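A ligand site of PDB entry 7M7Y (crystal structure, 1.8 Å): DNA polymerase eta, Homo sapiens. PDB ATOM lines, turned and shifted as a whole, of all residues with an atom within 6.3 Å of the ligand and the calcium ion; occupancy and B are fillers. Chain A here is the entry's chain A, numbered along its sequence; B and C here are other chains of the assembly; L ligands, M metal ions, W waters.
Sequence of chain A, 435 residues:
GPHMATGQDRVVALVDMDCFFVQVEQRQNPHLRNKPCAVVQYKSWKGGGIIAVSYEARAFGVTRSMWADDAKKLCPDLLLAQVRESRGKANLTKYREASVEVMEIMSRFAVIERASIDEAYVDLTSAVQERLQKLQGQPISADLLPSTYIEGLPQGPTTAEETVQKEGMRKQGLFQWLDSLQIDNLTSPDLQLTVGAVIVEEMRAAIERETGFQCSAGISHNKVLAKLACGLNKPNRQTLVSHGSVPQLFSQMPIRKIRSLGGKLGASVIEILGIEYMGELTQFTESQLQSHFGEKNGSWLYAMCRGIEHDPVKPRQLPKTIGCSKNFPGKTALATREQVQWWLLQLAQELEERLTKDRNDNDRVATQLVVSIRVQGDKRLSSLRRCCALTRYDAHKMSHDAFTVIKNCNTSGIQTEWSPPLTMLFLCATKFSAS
O2 of the ligand sits at hydrogen-bond distance from OH of Tyr 55 (2.6 Å).
O4 of DT 3 of chain B sits at hydrogen-bond distance from N3 of the ligand.
The backbone NH (N) of Cys 19 lies within hydrogen-bond range of an oxygen (O2) of the ligand (2.8 Å).
The side-chain amino group (NZ) of Lys 234 is in salt-bridge range of an oxygen (O1) of the ligand, at 3.6 Å.
NH1 of Arg 58 is in salt-bridge range of O1 of the ligand (3.1 Å).
O5 of the ligand is in salt-bridge range of NH2 of Arg 64.
O12 of the ligand lies within hydrogen-bond range of N of Phe 21 (3.0 Å).
The backbone NH of Phe 20 sits at hydrogen-bond distance from an oxygen (O12) of the ligand (3.4 Å).
N6 of DA 8 of chain C lies close to a nitrogen (N3) of the ligand (3.5 Å).
O4 of DT 2 of chain B lies within hydrogen-bond range of N3 of the ligand (3.4 Å).
OD2 of Asp 16 lies within salt-bridge range of NZ of Lys 234 (2.9 Å).
OD1 of Asp 118 sits at hydrogen-bond distance from OG of Ser 116, at 3.4 Å.
OH of Tyr 55 lies close to NH1 of Arg 58 (3.2 Å).
O2 of DT 3 of chain B is in hydrogen-bond range of the side-chain amide nitrogen of Gln 41 (3.0 Å).
NE of Arg 58 is in hydrogen-bond range of O of Val 53, at 2.9 Å.
The backbone carbonyl oxygen of Ile 51 sits at hydrogen-bond distance from the guanidinium group of Arg 64 (2.8 Å).
O3' of DA 8 of chain C is in hydrogen-bond range of the side-chain hydroxyl of Ser 116, 2.4 Å away.
Asp 18 touches the ligand (CA to O2, 3.4 Å).
O of Ile 51 touches C4 of the ligand (3.4 Å).
Ala 52 touches the ligand (CB to O12, 3.6 Å).
CG2 of Ile 117 touches O11 of the ligand, 3.9 Å away.
DT 4 of chain B touches the ligand.
Hydrophobic or aromatic side chains that line the ligand: Phe 20, Phe 21, Ile 51, Ala 52, Tyr 55 and Ile 117.
Of the 24 residues printed, 18 come within 4 Å of the ligand.
Along chain A the residues within 4 Å of the ligand span positions 16 to 234.
The nearest printed residue that does not touch the ligand is Glu 119 (4.04 Å).
Within 4 Å of the calcium ion: Asp 16, Met 17 and Asp 118.
The side-chain carboxylate (OD1) of Asp 16 is bound to the calcium ion (2.3 Å).
O of Met 17 binds the calcium ion (2.3 Å).
The side-chain carboxylate (OD2) of Asp 118 is bound to the calcium ion (2.3 Å).
O3 of the ligand is bound to the calcium ion (2.3 Å).
O4 of the ligand is bound to the calcium ion, at 2.3 Å.
O8 of the ligand is bound to the calcium ion, 2.4 Å away.
Water W3 bridges N3 of DA 8 of chain C and an oxygen (O11) of the ligand.
Water W5 lies within hydrogen-bond range of the side-chain carboxylate of Asp 16 (2.7 Å) and the side-chain carboxylate of Glu 119 (2.7 Å).
Water W7 bridges a nitrogen (N2) of the ligand (2.8 Å) and the guanidinium group of Arg 64 (3.2 Å).
Water W8 lies within hydrogen-bond range of the side-chain hydroxyl of Tyr 55 (3.1 Å), the guanidinium group of Arg 58 (3.3 Å) and an oxygen (O1) of the ligand (3.4 Å).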
ATOM      1  N   ASP A  16     -32.032 -21.763   4.761  1.00  0.00           N
ATOM      2  CA  ASP A  16     -30.733 -22.243   5.218  1.00  0.00           C
ATOM      3  C   ASP A  16     -30.127 -21.111   6.055  1.00  0.00           C
ATOM      4  O   ASP A  16     -29.807 -20.045   5.518  1.00  0.00           O
ATOM      5  CB  ASP A  16     -29.863 -22.542   3.998  1.00  0.00           C
ATOM      6  CG  ASP A  16     -28.588 -23.261   4.309  1.00  0.00           C
ATOM      7  OD1 ASP A  16     -28.154 -23.258   5.471  1.00  0.00           O
ATOM      8  OD2 ASP A  16     -27.992 -23.819   3.352  1.00  0.00           O
ATOM      9  N   MET A  17     -29.969 -21.305   7.369  1.00  0.00           N
ATOM     10  CA  MET A  17     -29.395 -20.233   8.188  1.00  0.00           C
ATOM     11  C   MET A  17     -27.955 -19.967   7.753  1.00  0.00           C
ATOM     12  O   MET A  17     -27.219 -20.895   7.407  1.00  0.00           O
ATOM     13  CB  MET A  17     -29.438 -20.571   9.685  1.00  0.00           C
ATOM     14  CG  MET A  17     -30.789 -21.018  10.274  1.00  0.00           C
ATOM     15  SD  MET A  17     -32.093 -19.843   9.880  1.00  0.00           S
ATOM     16  CE  MET A  17     -31.599 -18.427  10.828  1.00  0.00           C
ATOM     17  N   ASP A  18     -27.558 -18.707   7.730  1.00  0.00           N
ATOM     18  CA  ASP A  18     -26.182 -18.380   7.384  1.00  0.00           C
ATOM     19  C   ASP A  18     -25.256 -18.673   8.555  1.00  0.00           C
ATOM     20  O   ASP A  18     -25.580 -18.353   9.696  1.00  0.00           O
ATOM     21  CB  ASP A  18     -26.084 -16.909   6.990  1.00  0.00           C
ATOM     22  CG  ASP A  18     -26.930 -16.560   5.758  1.00  0.00           C
ATOM     23  OD1 ASP A  18     -27.079 -17.413   4.855  1.00  0.00           O
ATOM     24  OD2 ASP A  18     -27.440 -15.435   5.712  1.00  0.00           O
ATOM     25  N   CYS A  19     -24.080 -19.264   8.256  1.00  0.00           N
ATOM     26  CA  CYS A  19     -23.047 -19.595   9.246  1.00  0.00           C
ATOM     27  C   CYS A  19     -23.640 -19.790  10.634  1.00  0.00           C
ATOM     28  O   CYS A  19     -23.379 -19.003  11.554  1.00  0.00           O
ATOM     29  CB  CYS A  19     -21.921 -18.539   9.297  1.00  0.00           C
ATOM     30  SG  CYS A  19     -22.354 -16.829   9.537  1.00  0.00           S
ATOM     31  N   PHE A  20     -24.499 -20.809  10.774  1.00  0.00           N
ATOM     32  CA  PHE A  20     -25.466 -20.840  11.868  1.00  0.00           C
ATOM     33  C   PHE A  20     -24.830 -20.832  13.255  1.00  0.00           C
ATOM     34  O   PHE A  20     -25.220 -20.030  14.124  1.00  0.00           O
ATOM     35  CB  PHE A  20     -26.367 -22.064  11.721  1.00  0.00           C
ATOM     36  CG  PHE A  20     -27.447 -22.124  12.744  1.00  0.00           C
ATOM     37  CD1 PHE A  20     -28.269 -21.032  12.979  1.00  0.00           C
ATOM     38  CD2 PHE A  20     -27.632 -23.276  13.490  1.00  0.00           C
ATOM     39  CE1 PHE A  20     -29.269 -21.094  13.948  1.00  0.00           C
ATOM     40  CE2 PHE A  20     -28.643 -23.345  14.454  1.00  0.00           C
ATOM     41  CZ  PHE A  20     -29.456 -22.250  14.685  1.00  0.00           C
ATOM     42  N   PHE A  21     -23.894 -21.749  13.525  1.00  0.00           N
ATOM     43  CA  PHE A  21     -23.351 -21.802  14.886  1.00  0.00           C
ATOM     44  C   PHE A  21     -22.632 -20.500  15.234  1.00  0.00           C
ATOM     45  O   PHE A  21     -22.627 -20.064  16.405  1.00  0.00           O
ATOM     46  CB  PHE A  21     -22.395 -22.988  15.084  1.00  0.00           C
ATOM     47  CG  PHE A  21     -23.049 -24.339  15.103  1.00  0.00           C
ATOM     48  CD1 PHE A  21     -24.354 -24.533  14.678  1.00  0.00           C
ATOM     49  CD2 PHE A  21     -22.328 -25.436  15.545  1.00  0.00           C
ATOM     50  CE1 PHE A  21     -24.921 -25.801  14.702  1.00  0.00           C
ATOM     51  CE2 PHE A  21     -22.895 -26.723  15.578  1.00  0.00           C
ATOM     52  CZ  PHE A  21     -24.198 -26.893  15.152  1.00  0.00           C
ATOM     53  N   VAL A  22     -21.998 -19.877  14.237  1.00  0.00           N
ATOM     54  CA  VAL A  22     -21.371 -18.579  14.425  1.00  0.00           C
ATOM     55  C   VAL A  22     -22.403 -17.538  14.821  1.00  0.00           C
ATOM     56  O   VAL A  22     -22.175 -16.736  15.731  1.00  0.00           O
ATOM     57  CB  VAL A  22     -20.607 -18.138  13.155  1.00  0.00           C
ATOM     58  CG1 VAL A  22     -20.254 -16.631  13.210  1.00  0.00           C
ATOM     59  CG2 VAL A  22     -19.362 -18.990  12.953  1.00  0.00           C
ATOM     60  N   GLN A  41     -14.477 -26.942  18.082  1.00  0.00           N
ATOM     61  CA  GLN A  41     -14.694 -27.992  19.072  1.00  0.00           C
ATOM     62  C   GLN A  41     -13.353 -28.419  19.641  1.00  0.00           C
ATOM     63  O   GLN A  41     -12.413 -28.690  18.886  1.00  0.00           O
ATOM     64  CB  GLN A  41     -15.387 -29.219  18.480  1.00  0.00           C
ATOM     65  CG  GLN A  41     -16.759 -28.967  17.907  1.00  0.00           C
ATOM     66  CD  GLN A  41     -17.483 -30.261  17.555  1.00  0.00           C
ATOM     67  OE1 GLN A  41     -18.575 -30.524  18.074  1.00  0.00           O
ATOM     68  NE2 GLN A  41     -16.890 -31.069  16.673  1.00  0.00           N
ATOM     69  N   ILE A  51     -15.768 -25.897  13.041  1.00  0.00           N
ATOM     70  CA  ILE A  51     -17.007 -26.430  12.488  1.00  0.00           C
ATOM     71  C   ILE A  51     -17.892 -25.347  11.898  1.00  0.00           C
ATOM     72  O   ILE A  51     -18.857 -25.687  11.186  1.00  0.00           O
ATOM     73  CB  ILE A  51     -17.802 -27.272  13.514  1.00  0.00           C
ATOM     74  CG1 ILE A  51     -18.210 -26.439  14.731  1.00  0.00           C
ATOM     75  CG2 ILE A  51     -16.993 -28.508  13.938  1.00  0.00           C
ATOM     76  CD1 ILE A  51     -19.175 -27.214  15.637  1.00  0.00           C
ATOM     77  N   ALA A  52     -17.590 -24.066  12.120  1.00  0.00           N
ATOM     78  CA  ALA A  52     -18.412 -23.028  11.481  1.00  0.00           C
ATOM     79  C   ALA A  52     -17.592 -21.764  11.349  1.00  0.00           C
ATOM     80  O   ALA A  52     -16.770 -21.476  12.217  1.00  0.00           O
ATOM     81  CB  ALA A  52     -19.703 -22.744  12.259  1.00  0.00           C
ATOM     82  N   VAL A  53     -17.837 -20.991  10.286  1.00  0.00           N
ATOM     83  CA  VAL A  53     -16.965 -19.875   9.917  1.00  0.00           C
ATOM     84  C   VAL A  53     -17.768 -18.674   9.454  1.00  0.00           C
ATOM     85  O   VAL A  53     -18.605 -18.804   8.552  1.00  0.00           O
ATOM     86  CB  VAL A  53     -16.003 -20.274   8.773  1.00  0.00           C
ATOM     87  CG1 VAL A  53     -14.996 -19.160   8.522  1.00  0.00           C
ATOM     88  CG2 VAL A  53     -15.283 -21.555   9.114  1.00  0.00           C
ATOM     89  N   TYR A  55     -18.605 -15.189   7.483  1.00  0.00           N
ATOM     90  CA  TYR A  55     -18.250 -14.789   6.117  1.00  0.00           C
ATOM     91  C   TYR A  55     -17.031 -13.873   6.079  1.00  0.00           C
ATOM     92  O   TYR A  55     -16.215 -13.934   5.141  1.00  0.00           O
ATOM     93  CB  TYR A  55     -19.471 -14.179   5.421  1.00  0.00           C
ATOM     94  CG  TYR A  55     -20.432 -15.269   4.964  1.00  0.00           C
ATOM     95  CD1 TYR A  55     -21.280 -15.902   5.859  1.00  0.00           C
ATOM     96  CD2 TYR A  55     -20.417 -15.717   3.644  1.00  0.00           C
ATOM     97  CE1 TYR A  55     -22.127 -16.941   5.439  1.00  0.00           C
ATOM     98  CE2 TYR A  55     -21.244 -16.745   3.225  1.00  0.00           C
ATOM     99  CZ  TYR A  55     -22.099 -17.357   4.122  1.00  0.00           C
ATOM    100  OH  TYR A  55     -22.927 -18.382   3.679  1.00  0.00           O
ATOM    101  N   ARG A  58     -14.267 -16.269   6.167  1.00  0.00           N
ATOM    102  CA  ARG A  58     -14.151 -17.005   4.892  1.00  0.00           C
ATOM    103  C   ARG A  58     -13.368 -16.196   3.863  1.00  0.00           C
ATOM    104  O   ARG A  58     -12.708 -16.794   2.992  1.00  0.00           O
ATOM    105  CB  ARG A  58     -15.525 -17.339   4.327  1.00  0.00           C
ATOM    106  CG  ARG A  58     -16.318 -18.254   5.195  1.00  0.00           C
ATOM    107  CD  ARG A  58     -17.698 -18.505   4.633  1.00  0.00           C
ATOM    108  NE  ARG A  58     -18.557 -19.066   5.667  1.00  0.00           N
ATOM    109  CZ  ARG A  58     -19.693 -19.702   5.444  1.00  0.00           C
ATOM    110  NH1 ARG A  58     -20.118 -19.864   4.200  1.00  0.00           N
ATOM    111  NH2 ARG A  58     -20.401 -20.186   6.468  1.00  0.00           N
ATOM    112  N   ARG A  64     -14.347 -24.777   7.263  1.00  0.00           N
ATOM    113  CA  ARG A  64     -14.662 -25.939   8.070  1.00  0.00           C
ATOM    114  C   ARG A  64     -13.611 -27.031   7.858  1.00  0.00           C
ATOM    115  O   ARG A  64     -12.992 -27.114   6.795  1.00  0.00           O
ATOM    116  CB  ARG A  64     -16.074 -26.408   7.701  1.00  0.00           C
ATOM    117  CG  ARG A  64     -16.541 -27.671   8.368  1.00  0.00           C
ATOM    118  CD  ARG A  64     -18.029 -27.883   8.115  1.00  0.00           C
ATOM    119  NE  ARG A  64     -18.821 -26.747   8.609  1.00  0.00           N
ATOM    120  CZ  ARG A  64     -19.779 -26.143   7.907  1.00  0.00           C
ATOM    121  NH1 ARG A  64     -20.076 -26.563   6.686  1.00  0.00           N
ATOM    122  NH2 ARG A  64     -20.441 -25.125   8.442  1.00  0.00           N
ATOM    123  N   SER A 116     -32.215 -30.349   8.471  1.00  0.00           N
ATOM    124  CA  SER A 116     -31.011 -30.439   9.291  1.00  0.00           C
ATOM    125  C   SER A 116     -31.164 -29.431  10.420  1.00  0.00           C
ATOM    126  O   SER A 116     -32.111 -28.629  10.423  1.00  0.00           O
ATOM    127  CB  SER A 116     -29.746 -30.203   8.465  1.00  0.00           C
ATOM    128  OG  SER A 116     -29.631 -28.832   8.131  1.00  0.00           O
ATOM    129  N   ILE A 117     -30.120 -29.327  11.248  1.00  0.00           N
ATOM    130  CA  ILE A 117     -30.182 -28.400  12.386  1.00  0.00           C
ATOM    131  C   ILE A 117     -30.483 -26.971  11.941  1.00  0.00           C
ATOM    132  O   ILE A 117     -31.061 -26.189  12.706  1.00  0.00           O
ATOM    133  CB  ILE A 117     -28.881 -28.436  13.210  1.00  0.00           C
ATOM    134  CG1 ILE A 117     -29.098 -27.795  14.595  1.00  0.00           C
ATOM    135  CG2 ILE A 117     -27.733 -27.737  12.471  1.00  0.00           C
ATOM    136  CD1 ILE A 117     -28.033 -28.224  15.629  1.00  0.00           C
ATOM    137  N   ASP A 118     -30.127 -26.602  10.707  1.00  0.00           N
ATOM    138  CA  ASP A 118     -30.379 -25.212  10.340  1.00  0.00           C
ATOM    139  C   ASP A 118     -31.016 -25.071   8.968  1.00  0.00           C
ATOM    140  O   ASP A 118     -30.992 -23.959   8.399  1.00  0.00           O
ATOM    141  CB  ASP A 118     -29.138 -24.324  10.358  1.00  0.00           C
ATOM    142  CG  ASP A 118     -28.189 -24.643   9.221  1.00  0.00           C
ATOM    143  OD1 ASP A 118     -28.381 -25.647   8.512  1.00  0.00           O
ATOM    144  OD2 ASP A 118     -27.487 -23.688   8.830  1.00  0.00           O
ATOM    145  N   GLU A 119     -31.602 -26.146   8.431  1.00  0.00           N
ATOM    146  CA  GLU A 119     -32.241 -26.074   7.130  1.00  0.00           C
ATOM    147  C   GLU A 119     -33.635 -26.650   7.230  1.00  0.00           C
ATOM    148  O   GLU A 119     -33.839 -27.720   7.845  1.00  0.00           O
ATOM    149  CB  GLU A 119     -31.472 -26.859   6.064  1.00  0.00           C
ATOM    150  CG  GLU A 119     -30.031 -26.403   5.865  1.00  0.00           C
ATOM    151  CD  GLU A 119     -29.413 -26.965   4.592  1.00  0.00           C
ATOM    152  OE1 GLU A 119     -30.118 -27.688   3.865  1.00  0.00           O
ATOM    153  OE2 GLU A 119     -28.221 -26.672   4.321  1.00  0.00           O
ATOM    154  N   LYS A 234     -25.791 -16.570  -1.265  1.00  0.00           N
ATOM    155  CA  LYS A 234     -25.585 -16.288   0.156  1.00  0.00           C
ATOM    156  C   LYS A 234     -24.508 -15.241   0.375  1.00  0.00           C
ATOM    157  O   LYS A 234     -23.675 -14.996  -0.509  1.00  0.00           O
ATOM    158  CB  LYS A 234     -25.203 -17.549   0.920  1.00  0.00           C
ATOM    159  CG  LYS A 234     -25.858 -18.800   0.552  1.00  0.00           C
ATOM    160  CD  LYS A 234     -25.636 -19.709   1.762  1.00  0.00           C
ATOM    161  CE  LYS A 234     -26.243 -21.071   1.567  1.00  0.00           C
ATOM    162  NZ  LYS A 234     -25.878 -22.007   2.662  1.00  0.00           N
ATOM    163  N   PRO A 235     -24.488 -14.575   1.559  1.00  0.00           N
ATOM    164  CA  PRO A 235     -25.541 -14.777   2.580  1.00  0.00           C
ATOM    165  C   PRO A 235     -26.644 -13.728   2.538  1.00  0.00           C
ATOM    166  O   PRO A 235     -26.590 -12.770   1.754  1.00  0.00           O
ATOM    167  CB  PRO A 235     -24.743 -14.677   3.889  1.00  0.00           C
ATOM    168  CG  PRO A 235     -23.706 -13.632   3.575  1.00  0.00           C
ATOM    169  CD  PRO A 235     -23.350 -13.814   2.098  1.00  0.00           C
ATOM    170  P    DT B   2      -7.162 -35.437  10.295  1.00  0.00           P
ATOM    171  OP1  DT B   2      -6.503 -36.606   9.655  1.00  0.00           O
ATOM    172  OP2  DT B   2      -6.757 -34.046   9.981  1.00  0.00           O
ATOM    173  O5'  DT B   2      -8.720 -35.628   9.978  1.00  0.00           O
ATOM    174  C5'  DT B   2      -9.687 -34.533   9.994  1.00  0.00           C
ATOM    175  C4'  DT B   2      -9.986 -34.239  11.431  1.00  0.00           C
ATOM    176  O4'  DT B   2     -10.765 -32.977  11.462  1.00  0.00           O
ATOM    177  C3'  DT B   2     -10.897 -35.289  12.052  1.00  0.00           C
ATOM    178  O3'  DT B   2     -10.552 -35.437  13.410  1.00  0.00           O
ATOM    179  C2'  DT B   2     -12.290 -34.706  11.831  1.00  0.00           C
ATOM    180  C1'  DT B   2     -12.080 -33.204  11.948  1.00  0.00           C
ATOM    181  N1   DT B   2     -13.099 -32.446  11.078  1.00  0.00           N
ATOM    182  C2   DT B   2     -13.821 -31.364  11.582  1.00  0.00           C
ATOM    183  O2   DT B   2     -13.677 -30.917  12.712  1.00  0.00           O
ATOM    184  N3   DT B   2     -14.720 -30.802  10.691  1.00  0.00           N
ATOM    185  C4   DT B   2     -14.978 -31.211   9.385  1.00  0.00           C
ATOM    186  O4   DT B   2     -15.800 -30.647   8.671  1.00  0.00           O
ATOM    187  C5   DT B   2     -14.209 -32.355   8.936  1.00  0.00           C
ATOM    188  C7   DT B   2     -14.395 -32.878   7.545  1.00  0.00           C
ATOM    189  C6   DT B   2     -13.330 -32.905   9.791  1.00  0.00           C
ATOM    190  P    DT B   3     -11.420 -36.363  14.383  1.00  0.00           P
ATOM    191  OP1  DT B   3     -10.632 -36.814  15.556  1.00  0.00           O
ATOM    192  OP2  DT B   3     -11.959 -37.369  13.439  1.00  0.00           O
ATOM    193  O5'  DT B   3     -12.673 -35.494  14.764  1.00  0.00           O
ATOM    194  C5'  DT B   3     -12.546 -34.451  15.722  1.00  0.00           C
ATOM    195  C4'  DT B   3     -13.890 -34.166  16.329  1.00  0.00           C
ATOM    196  O4'  DT B   3     -14.681 -33.546  15.288  1.00  0.00           O
ATOM    197  C3'  DT B   3     -14.700 -35.384  16.781  1.00  0.00           C
ATOM    198  O3'  DT B   3     -15.356 -35.042  17.972  1.00  0.00           O
ATOM    199  C2'  DT B   3     -15.673 -35.616  15.621  1.00  0.00           C
ATOM    200  C1'  DT B   3     -15.923 -34.194  15.179  1.00  0.00           C
ATOM    201  N1   DT B   3     -16.336 -34.092  13.735  1.00  0.00           N
ATOM    202  C2   DT B   3     -17.234 -33.144  13.370  1.00  0.00           C
ATOM    203  O2   DT B   3     -17.767 -32.409  14.172  1.00  0.00           O
ATOM    204  N3   DT B   3     -17.517 -33.090  12.024  1.00  0.00           N
ATOM    205  C4   DT B   3     -16.982 -33.876  11.029  1.00  0.00           C
ATOM    206  O4   DT B   3     -17.310 -33.745   9.850  1.00  0.00           O
ATOM    207  C5   DT B   3     -16.018 -34.857  11.464  1.00  0.00           C
ATOM    208  C7   DT B   3     -15.370 -35.761  10.444  1.00  0.00           C
ATOM    209  C6   DT B   3     -15.728 -34.910  12.773  1.00  0.00           C
ATOM    210  P    DT B   4     -16.404 -36.027  18.674  1.00  0.00           P
ATOM    211  OP1  DT B   4     -16.305 -35.748  20.112  1.00  0.00           O
ATOM    212  OP2  DT B   4     -16.266 -37.412  18.164  1.00  0.00           O
ATOM    213  O5'  DT B   4     -17.810 -35.460  18.152  1.00  0.00           O
ATOM    214  C5'  DT B   4     -18.296 -34.199  18.607  1.00  0.00           C
ATOM    215  C4'  DT B   4     -19.707 -33.956  18.094  1.00  0.00           C
ATOM    216  O4'  DT B   4     -19.703 -33.820  16.655  1.00  0.00           O
ATOM    217  C3'  DT B   4     -20.708 -35.083  18.397  1.00  0.00           C
ATOM    218  O3'  DT B   4     -21.991 -34.528  18.660  1.00  0.00           O
ATOM    219  C2'  DT B   4     -20.707 -35.857  17.090  1.00  0.00           C
ATOM    220  C1'  DT B   4     -20.677 -34.685  16.118  1.00  0.00           C
ATOM    221  N1   DT B   4     -20.312 -35.047  14.722  1.00  0.00           N
ATOM    222  C2   DT B   4     -20.895 -34.340  13.675  1.00  0.00           C
ATOM    223  O2   DT B   4     -21.702 -33.435  13.843  1.00  0.00           O
ATOM    224  N3   DT B   4     -20.520 -34.733  12.432  1.00  0.00           N
ATOM    225  C4   DT B   4     -19.602 -35.724  12.108  1.00  0.00           C
ATOM    226  O4   DT B   4     -19.339 -36.004  10.938  1.00  0.00           O
ATOM    227  C5   DT B   4     -19.021 -36.424  13.233  1.00  0.00           C
ATOM    228  C7   DT B   4     -18.026 -37.541  13.003  1.00  0.00           C
ATOM    229  C6   DT B   4     -19.389 -36.053  14.474  1.00  0.00           C
ATOM    230  P    DA C   8     -25.290 -30.132   2.565  1.00  0.00           P
ATOM    231  OP1  DA C   8     -25.856 -29.044   1.764  1.00  0.00           O
ATOM    232  OP2  DA C   8     -23.814 -30.172   2.768  1.00  0.00           O
ATOM    233  O5'  DA C   8     -26.018 -30.153   3.999  1.00  0.00           O
ATOM    234  C5'  DA C   8     -25.722 -29.164   4.955  1.00  0.00           C
ATOM    235  C4'  DA C   8     -26.516 -29.356   6.230  1.00  0.00           C
ATOM    236  O4'  DA C   8     -26.217 -30.690   6.799  1.00  0.00           O
ATOM    237  C3'  DA C   8     -26.160 -28.366   7.321  1.00  0.00           C
ATOM    238  O3'  DA C   8     -27.285 -28.155   8.178  1.00  0.00           O
ATOM    239  C2'  DA C   8     -25.003 -29.066   8.057  1.00  0.00           C
ATOM    240  C1'  DA C   8     -25.407 -30.543   7.964  1.00  0.00           C
ATOM    241  N9   DA C   8     -24.272 -31.473   7.866  1.00  0.00           N
ATOM    242  C8   DA C   8     -23.740 -32.019   6.722  1.00  0.00           C
ATOM    243  N7   DA C   8     -22.737 -32.839   6.935  1.00  0.00           N
ATOM    244  C5   DA C   8     -22.601 -32.845   8.328  1.00  0.00           C
ATOM    245  C6   DA C   8     -21.720 -33.510   9.196  1.00  0.00           C
ATOM    246  N6   DA C   8     -20.758 -34.358   8.775  1.00  0.00           N
ATOM    247  N1   DA C   8     -21.853 -33.283  10.512  1.00  0.00           N
ATOM    248  C2   DA C   8     -22.809 -32.437  10.945  1.00  0.00           C
ATOM    249  N3   DA C   8     -23.697 -31.753  10.230  1.00  0.00           N
ATOM    250  C4   DA C   8     -23.536 -32.003   8.909  1.00  0.00           C
HETATM  251  P1  LIG L   1     -23.558 -21.398   5.426  1.00  0.00           P
HETATM  252  O1  LIG L   1     -22.685 -21.671   4.237  1.00  0.00           O
HETATM  253  O2  LIG L   1     -23.808 -19.945   5.558  1.00  0.00           O
HETATM  254  O3  LIG L   1     -24.823 -22.166   5.351  1.00  0.00           O
HETATM  255  P2  LIG L   1     -23.202 -22.891   7.813  1.00  0.00           P
HETATM  256  O4  LIG L   1     -24.584 -22.612   8.305  1.00  0.00           O
HETATM  257  O5  LIG L   1     -22.235 -22.785   8.937  1.00  0.00           O
HETATM  258  O6  LIG L   1     -22.791 -21.857   6.701  1.00  0.00           O
HETATM  259  P3  LIG L   1     -23.977 -25.513   7.143  1.00  0.00           P
HETATM  260  O7  LIG L   1     -23.376 -26.528   6.240  1.00  0.00           O
HETATM  261  O8  LIG L   1     -25.302 -25.112   6.641  1.00  0.00           O
HETATM  262  O9  LIG L   1     -23.045 -24.291   7.179  1.00  0.00           O
HETATM  263  O10 LIG L   1     -24.073 -26.075   8.598  1.00  0.00           O
HETATM  264  C1  LIG L   1     -24.906 -25.582   9.591  1.00  0.00           C
HETATM  265  C2  LIG L   1     -24.270 -25.803  10.948  1.00  0.00           C
HETATM  266  O11 LIG L   1     -24.086 -27.216  11.194  1.00  0.00           O
HETATM  267  C3  LIG L   1     -22.906 -25.127  10.989  1.00  0.00           C
HETATM  268  O12 LIG L   1     -23.028 -23.819  11.524  1.00  0.00           O
HETATM  269  C4  LIG L   1     -22.139 -26.028  11.929  1.00  0.00           C
HETATM  270  C5  LIG L   1     -22.750 -27.342  11.710  1.00  0.00           C
HETATM  271  N1  LIG L   1     -21.965 -28.199  10.805  1.00  0.00           N
HETATM  272  C6  LIG L   1     -21.947 -28.175   9.490  1.00  0.00           C
HETATM  273  N2  LIG L   1     -21.099 -29.099   9.033  1.00  0.00           N
HETATM  274  C7  LIG L   1     -20.581 -29.736  10.071  1.00  0.00           C
HETATM  275  C8  LIG L   1     -19.675 -30.753  10.216  1.00  0.00           C
HETATM  276  N3  LIG L   1     -19.124 -31.340   9.158  1.00  0.00           N
HETATM  277  N4  LIG L   1     -19.363 -31.143  11.431  1.00  0.00           N
HETATM  278  C9  LIG L   1     -19.908 -30.565  12.492  1.00  0.00           C
HETATM  279  N5  LIG L   1     -20.768 -29.594  12.441  1.00  0.00           N
HETATM  280  C10 LIG L   1     -21.117 -29.164  11.226  1.00  0.00           C
HETATM  281 CA    CA M   1     -26.415 -22.963   6.879  1.00  0.00          CA
HETATM  282  O   HOH W   1     -19.588 -22.223   8.400  1.00  0.00           O
HETATM  283  O   HOH W   2     -20.620 -23.441   4.091  1.00  0.00           O
HETATM  284  O   HOH W   3     -25.014 -29.757  11.493  1.00  0.00           O
HETATM  285  O   HOH W   4     -18.946 -31.166   6.196  1.00  0.00           O
HETATM  286  O   HOH W   5     -25.930 -25.387   3.911  1.00  0.00           O
HETATM  287  O   HOH W   6     -22.414 -29.927  14.769  1.00  0.00           O
HETATM  288  O   HOH W   7     -21.984 -29.164   6.338  1.00  0.00           O
HETATM  289  O   HOH W   8     -21.792 -20.079   1.343  1.00  0.00           O
